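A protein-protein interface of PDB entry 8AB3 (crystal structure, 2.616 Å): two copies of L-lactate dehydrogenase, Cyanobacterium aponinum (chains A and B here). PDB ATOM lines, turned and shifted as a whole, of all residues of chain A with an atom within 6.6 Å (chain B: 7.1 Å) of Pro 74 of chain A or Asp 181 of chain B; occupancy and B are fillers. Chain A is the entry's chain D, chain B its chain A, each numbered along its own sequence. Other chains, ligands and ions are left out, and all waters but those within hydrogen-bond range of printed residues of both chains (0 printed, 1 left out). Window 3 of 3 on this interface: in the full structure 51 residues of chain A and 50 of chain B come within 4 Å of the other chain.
Of the 11 printed residues of chain A, 4 touch a printed residue of chain B. Hydrophobic or aromatic side chains of chain A that line the printed part of chain B: Pro 70 and Pro 74. Of the 11 printed residues of chain B, 3 touch a printed residue of chain A. Hydrophobic or aromatic side chains of chain B that line the printed part of chain A: Pro 182. Among the printed residues, 6 pairs touch across the chains. Among the printed residues, no Asp or Glu carboxylate lies within 4 Å of a Lys or Arg side-chain nitrogen of the other chain.
Pro 74 of chain A touches just these residues of chain B: Asp 181 (3.3 Å) and Arg 183 (3.5 Å). Printed residues of chain B within 4 Å of Ile 72 of chain A: Arg 183. Of the printed residues of chain B, Pro 70 of chain A touches Pro 182 and Arg 183. Printed residues of chain B within 4 Å of Pro 73 of chain A: Arg 183. Printed residues of chain A within 4 Å of Arg 183 of chain B: Pro 70, Ile 72, Pro 73 and Pro 74. Ile 180 of chain B touches none of the printed residues of chain A. Thr 75 of chain A touches none of the printed residues of chain B. The nearest residue of chain B that does not touch Pro 74 of chain A is Pro 182 of chain B (4.6 Å). The nearest residue of chain A that does not touch Asp 181 of chain B is Ile 72 of chain A (5.1 Å).
No position is printed for both chains. Of the 6 pairs that touch across the chains among the printed residues, none has its exchanged pair printed and touching as well.
OD2 of Asp 181 of chain B is in salt-bridge range of NH2 of Arg 183 of chain B, 3.0 Å away.
Pro 70 of chain A touches Pro 182 of chain B (CG to CB, 3.7 Å). CG of Arg 183 of chain B touches O of Pro 70 of chain A, 3.4 Å away. Arg 183 of chain B touches Ile 72 of chain A. Pro 73 of chain A touches Arg 183 of chain B. Asp 181 of chain B touches Pro 74 of chain A. Arg 183 of chain B touches Pro 74 of chain A (NH2 to CD, 3.5 Å).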
ATOM      1  N   LEU A  40      -2.402   0.977  -8.616  1.00  0.00           N
ATOM      2  CA  LEU A  40      -1.372   0.280  -7.840  1.00  0.00           C
ATOM      3  C   LEU A  40      -2.007  -0.800  -6.983  1.00  0.00           C
ATOM      4  O   LEU A  40      -1.502  -1.916  -6.948  1.00  0.00           O
ATOM      5  CB  LEU A  40      -0.583   1.241  -6.940  1.00  0.00           C
ATOM      6  CG  LEU A  40       0.378   2.179  -7.642  1.00  0.00           C
ATOM      7  CD1 LEU A  40       0.850   3.264  -6.696  1.00  0.00           C
ATOM      8  CD2 LEU A  40       1.523   1.418  -8.279  1.00  0.00           C
ATOM      9  N   ASP A  43      -3.057  -3.719  -9.104  1.00  0.00           N
ATOM     10  CA  ASP A  43      -1.887  -4.263  -9.812  1.00  0.00           C
ATOM     11  C   ASP A  43      -2.026  -4.301 -11.350  1.00  0.00           C
ATOM     12  O   ASP A  43      -1.775  -5.336 -11.971  1.00  0.00           O
ATOM     13  CB  ASP A  43      -1.510  -5.646  -9.249  1.00  0.00           C
ATOM     14  CG  ASP A  43      -0.100  -6.107  -9.603  1.00  0.00           C
ATOM     15  OD1 ASP A  43       0.767  -5.226  -9.920  1.00  0.00           O
ATOM     16  OD2 ASP A  43       0.145  -7.342  -9.579  1.00  0.00           O
ATOM     17  N   PHE A  45      -0.255  -2.477 -13.860  1.00  0.00           N
ATOM     18  CA  PHE A  45       0.988  -2.454 -14.605  1.00  0.00           C
ATOM     19  C   PHE A  45       2.157  -3.113 -13.895  1.00  0.00           C
ATOM     20  O   PHE A  45       2.166  -3.270 -12.673  1.00  0.00           O
ATOM     21  CB  PHE A  45       1.364  -0.985 -14.928  1.00  0.00           C
ATOM     22  CG  PHE A  45       0.326  -0.229 -15.717  1.00  0.00           C
ATOM     23  CD1 PHE A  45       0.312  -0.279 -17.100  1.00  0.00           C
ATOM     24  CD2 PHE A  45      -0.653   0.503 -15.074  1.00  0.00           C
ATOM     25  CE1 PHE A  45      -0.662   0.380 -17.821  1.00  0.00           C
ATOM     26  CE2 PHE A  45      -1.622   1.172 -15.801  1.00  0.00           C
ATOM     27  CZ  PHE A  45      -1.616   1.113 -17.168  1.00  0.00           C
ATOM     28  N   ASP A  46       3.172  -3.468 -14.679  1.00  0.00           N
ATOM     29  CA  ASP A  46       4.433  -3.973 -14.158  1.00  0.00           C
ATOM     30  C   ASP A  46       5.293  -2.752 -13.808  1.00  0.00           C
ATOM     31  O   ASP A  46       5.928  -2.750 -12.765  1.00  0.00           O
ATOM     32  CB  ASP A  46       5.106  -4.895 -15.182  1.00  0.00           C
ATOM     33  CG  ASP A  46       4.322  -6.174 -15.428  1.00  0.00           C
ATOM     34  OD1 ASP A  46       3.534  -6.574 -14.539  1.00  0.00           O
ATOM     35  OD2 ASP A  46       4.486  -6.769 -16.508  1.00  0.00           O
ATOM     36  N   MET A  69       4.104  -0.297  -1.019  1.00  0.00           N
ATOM     37  CA  MET A  69       4.326  -1.496  -1.829  1.00  0.00           C
ATOM     38  C   MET A  69       4.340  -2.813  -1.052  1.00  0.00           C
ATOM     39  O   MET A  69       3.773  -3.777  -1.564  1.00  0.00           O
ATOM     40  CB  MET A  69       5.592  -1.392  -2.691  1.00  0.00           C
ATOM     41  CG  MET A  69       5.411  -0.541  -3.917  1.00  0.00           C
ATOM     42  SD  MET A  69       4.141  -1.137  -5.063  1.00  0.00           S
ATOM     43  CE  MET A  69       3.272   0.333  -5.298  1.00  0.00           C
ATOM     44  N   PRO A  70       4.947  -2.912   0.156  1.00  0.00           N
ATOM     45  CA  PRO A  70       4.922  -4.195   0.866  1.00  0.00           C
ATOM     46  C   PRO A  70       3.518  -4.717   1.182  1.00  0.00           C
ATOM     47  O   PRO A  70       3.366  -5.915   1.432  1.00  0.00           O
ATOM     48  CB  PRO A  70       5.720  -3.906   2.144  1.00  0.00           C
ATOM     49  CG  PRO A  70       6.590  -2.743   1.795  1.00  0.00           C
ATOM     50  CD  PRO A  70       5.718  -1.905   0.917  1.00  0.00           C
ATOM     51  N   ILE A  72       0.857  -4.592  -0.973  1.00  0.00           N
ATOM     52  CA  ILE A  72       0.210  -4.999  -2.228  1.00  0.00           C
ATOM     53  C   ILE A  72       1.208  -5.719  -3.181  1.00  0.00           C
ATOM     54  O   ILE A  72       2.418  -5.695  -2.928  1.00  0.00           O
ATOM     55  CB  ILE A  72      -0.383  -3.723  -2.909  1.00  0.00           C
ATOM     56  CG1 ILE A  72       0.695  -2.639  -3.109  1.00  0.00           C
ATOM     57  CG2 ILE A  72      -1.603  -3.178  -2.165  1.00  0.00           C
ATOM     58  CD1 ILE A  72       0.266  -1.449  -3.914  1.00  0.00           C
ATOM     59  N   PRO A  73       0.750  -6.348  -4.296  1.00  0.00           N
ATOM     60  CA  PRO A  73       1.723  -6.921  -5.250  1.00  0.00           C
ATOM     61  C   PRO A  73       2.520  -5.772  -5.901  1.00  0.00           C
ATOM     62  O   PRO A  73       2.029  -4.644  -6.017  1.00  0.00           O
ATOM     63  CB  PRO A  73       0.853  -7.706  -6.250  1.00  0.00           C
ATOM     64  CG  PRO A  73      -0.535  -7.702  -5.687  1.00  0.00           C
ATOM     65  CD  PRO A  73      -0.634  -6.489  -4.797  1.00  0.00           C
ATOM     66  N   PRO A  74       3.792  -6.015  -6.253  1.00  0.00           N
ATOM     67  CA  PRO A  74       4.643  -4.918  -6.712  1.00  0.00           C
ATOM     68  C   PRO A  74       4.426  -4.370  -8.124  1.00  0.00           C
ATOM     69  O   PRO A  74       4.003  -5.059  -9.060  1.00  0.00           O
ATOM     70  CB  PRO A  74       6.047  -5.497  -6.577  1.00  0.00           C
ATOM     71  CG  PRO A  74       5.858  -6.940  -6.777  1.00  0.00           C
ATOM     72  CD  PRO A  74       4.553  -7.268  -6.125  1.00  0.00           C
ATOM     73  N   THR A  75       4.781  -3.085  -8.256  1.00  0.00           N
ATOM     74  CA  THR A  75       4.786  -2.301  -9.485  1.00  0.00           C
ATOM     75  C   THR A  75       5.958  -1.343  -9.392  1.00  0.00           C
ATOM     76  O   THR A  75       6.157  -0.715  -8.353  1.00  0.00           O
ATOM     77  CB  THR A  75       3.479  -1.525  -9.658  1.00  0.00           C
ATOM     78  OG1 THR A  75       2.421  -2.455  -9.922  1.00  0.00           O
ATOM     79  CG2 THR A  75       3.554  -0.498 -10.780  1.00  0.00           C
ATOM     80  N   ASP A  76       6.748  -1.241 -10.463  1.00  0.00           N
ATOM     81  CA  ASP A  76       7.862  -0.319 -10.500  1.00  0.00           C
ATOM     82  C   ASP A  76       7.307   1.077 -10.741  1.00  0.00           C
ATOM     83  O   ASP A  76       7.135   1.489 -11.884  1.00  0.00           O
ATOM     84  CB  ASP A  76       8.862  -0.705 -11.586  1.00  0.00           C
ATOM     85  CG  ASP A  76      10.183   0.039 -11.519  1.00  0.00           C
ATOM     86  OD1 ASP A  76      10.425   0.736 -10.507  1.00  0.00           O
ATOM     87  OD2 ASP A  76      10.979  -0.081 -12.476  1.00  0.00           O
ATOM     88  N   ARG B 171      11.739  -1.877   4.514  1.00  0.00           N
ATOM     89  CA  ARG B 171      11.708  -2.946   3.529  1.00  0.00           C
ATOM     90  C   ARG B 171      11.762  -2.434   2.098  1.00  0.00           C
ATOM     91  O   ARG B 171      12.397  -3.063   1.265  1.00  0.00           O
ATOM     92  CB  ARG B 171      10.464  -3.810   3.734  1.00  0.00           C
ATOM     93  CG  ARG B 171      10.553  -4.609   5.012  1.00  0.00           C
ATOM     94  CD  ARG B 171       9.264  -5.312   5.357  1.00  0.00           C
ATOM     95  NE  ARG B 171       9.425  -6.086   6.588  1.00  0.00           N
ATOM     96  CZ  ARG B 171       8.848  -7.258   6.822  1.00  0.00           C
ATOM     97  NH1 ARG B 171       8.059  -7.811   5.907  1.00  0.00           N
ATOM     98  NH2 ARG B 171       9.066  -7.894   7.967  1.00  0.00           N
ATOM     99  N   ALA B 175      14.805  -3.112  -0.402  1.00  0.00           N
ATOM    100  CA  ALA B 175      14.405  -3.789  -1.642  1.00  0.00           C
ATOM    101  C   ALA B 175      14.799  -2.999  -2.901  1.00  0.00           C
ATOM    102  O   ALA B 175      15.027  -3.609  -3.939  1.00  0.00           O
ATOM    103  CB  ALA B 175      12.914  -4.050  -1.649  1.00  0.00           C
ATOM    104  N   MET B 178      18.412  -3.857  -3.680  1.00  0.00           N
ATOM    105  CA  MET B 178      18.554  -5.207  -4.230  1.00  0.00           C
ATOM    106  C   MET B 178      17.731  -5.469  -5.489  1.00  0.00           C
ATOM    107  O   MET B 178      17.925  -6.496  -6.129  1.00  0.00           O
ATOM    108  CB  MET B 178      18.224  -6.246  -3.155  1.00  0.00           C
ATOM    109  CG  MET B 178      19.300  -6.358  -2.123  1.00  0.00           C
ATOM    110  SD  MET B 178      18.878  -7.311  -0.649  1.00  0.00           S
ATOM    111  CE  MET B 178      17.508  -6.401  -0.040  1.00  0.00           C
ATOM    112  N   ASP B 179      16.822  -4.553  -5.839  1.00  0.00           N
ATOM    113  CA  ASP B 179      15.901  -4.633  -6.971  1.00  0.00           C
ATOM    114  C   ASP B 179      14.997  -5.867  -6.882  1.00  0.00           C
ATOM    115  O   ASP B 179      14.864  -6.621  -7.842  1.00  0.00           O
ATOM    116  CB  ASP B 179      16.630  -4.526  -8.317  1.00  0.00           C
ATOM    117  CG  ASP B 179      15.735  -4.149  -9.486  1.00  0.00           C
ATOM    118  OD1 ASP B 179      14.538  -3.829  -9.249  1.00  0.00           O
ATOM    119  OD2 ASP B 179      16.225  -4.181 -10.645  1.00  0.00           O
ATOM    120  N   ILE B 180      14.389  -6.079  -5.706  1.00  0.00           N
ATOM    121  CA  ILE B 180      13.498  -7.222  -5.453  1.00  0.00           C
ATOM    122  C   ILE B 180      12.119  -6.746  -4.903  1.00  0.00           C
ATOM    123  O   ILE B 180      11.929  -5.558  -4.641  1.00  0.00           O
ATOM    124  CB  ILE B 180      14.198  -8.230  -4.479  1.00  0.00           C
ATOM    125  CG1 ILE B 180      14.532  -7.559  -3.133  1.00  0.00           C
ATOM    126  CG2 ILE B 180      15.424  -8.863  -5.111  1.00  0.00           C
ATOM    127  CD1 ILE B 180      14.959  -8.505  -2.068  1.00  0.00           C
ATOM    128  N   ASP B 181      11.165  -7.682  -4.732  1.00  0.00           N
ATOM    129  CA  ASP B 181       9.848  -7.418  -4.162  1.00  0.00           C
ATOM    130  C   ASP B 181      10.038  -7.083  -2.671  1.00  0.00           C
ATOM    131  O   ASP B 181      10.621  -7.879  -1.937  1.00  0.00           O
ATOM    132  CB  ASP B 181       8.993  -8.696  -4.288  1.00  0.00           C
ATOM    133  CG  ASP B 181       7.495  -8.545  -4.072  1.00  0.00           C
ATOM    134  OD1 ASP B 181       7.089  -7.640  -3.321  1.00  0.00           O
ATOM    135  OD2 ASP B 181       6.731  -9.345  -4.643  1.00  0.00           O
ATOM    136  N   PRO B 182       9.515  -5.935  -2.194  1.00  0.00           N
ATOM    137  CA  PRO B 182       9.622  -5.611  -0.754  1.00  0.00           C
ATOM    138  C   PRO B 182       9.022  -6.676   0.175  1.00  0.00           C
ATOM    139  O   PRO B 182       9.433  -6.783   1.330  1.00  0.00           O
ATOM    140  CB  PRO B 182       8.862  -4.290  -0.629  1.00  0.00           C
ATOM    141  CG  PRO B 182       8.853  -3.716  -2.003  1.00  0.00           C
ATOM    142  CD  PRO B 182       8.800  -4.879  -2.937  1.00  0.00           C
ATOM    143  N   ARG B 183       8.064  -7.489  -0.331  1.00  0.00           N
ATOM    144  CA  ARG B 183       7.466  -8.588   0.430  1.00  0.00           C
ATOM    145  C   ARG B 183       8.468  -9.733   0.707  1.00  0.00           C
ATOM    146  O   ARG B 183       8.220 -10.558   1.585  1.00  0.00           O
ATOM    147  CB  ARG B 183       6.193  -9.103  -0.255  1.00  0.00           C
ATOM    148  CG  ARG B 183       5.175  -8.002  -0.530  1.00  0.00           C
ATOM    149  CD  ARG B 183       3.962  -8.484  -1.308  1.00  0.00           C
ATOM    150  NE  ARG B 183       4.338  -9.106  -2.578  1.00  0.00           N
ATOM    151  CZ  ARG B 183       3.508  -9.791  -3.359  1.00  0.00           C
ATOM    152  NH1 ARG B 183       2.229  -9.921  -3.029  1.00  0.00           N
ATOM    153  NH2 ARG B 183       3.949 -10.339  -4.484  1.00  0.00           N
ATOM    154  N   SER B 184       9.602  -9.763  -0.022  1.00  0.00           N
ATOM    155  CA  SER B 184      10.690 -10.726   0.160  1.00  0.00           C
ATOM    156  C   SER B 184      11.783 -10.212   1.132  1.00  0.00           C
ATOM    157  O   SER B 184      12.703 -10.961   1.451  1.00  0.00           O
ATOM    158  CB  SER B 184      11.316 -11.097  -1.183  1.00  0.00           C
ATOM    159  OG  SER B 184      10.393 -11.735  -2.047  1.00  0.00           O
ATOM    160  N   VAL B 185      11.692  -8.954   1.590  1.00  0.00           N
ATOM    161  CA  VAL B 185      12.630  -8.374   2.544  1.00  0.00           C
ATOM    162  C   VAL B 185      12.006  -8.476   3.926  1.00  0.00           C
ATOM    163  O   VAL B 185      10.904  -7.973   4.127  1.00  0.00           O
ATOM    164  CB  VAL B 185      12.946  -6.899   2.222  1.00  0.00           C
ATOM    165  CG1 VAL B 185      13.833  -6.291   3.301  1.00  0.00           C
ATOM    166  CG2 VAL B 185      13.583  -6.762   0.849  1.00  0.00           C
ATOM    167  N   VAL B 206      17.038 -11.410   3.921  1.00  0.00           N
ATOM    168  CA  VAL B 206      16.320 -11.747   2.697  1.00  0.00           C
ATOM    169  C   VAL B 206      16.571 -13.223   2.439  1.00  0.00           C
ATOM    170  O   VAL B 206      17.719 -13.653   2.405  1.00  0.00           O
ATOM    171  CB  VAL B 206      16.629 -10.870   1.453  1.00  0.00           C
ATOM    172  CG1 VAL B 206      16.252  -9.414   1.691  1.00  0.00           C
ATOM    173  CG2 VAL B 206      18.077 -10.981   1.024  1.00  0.00           C
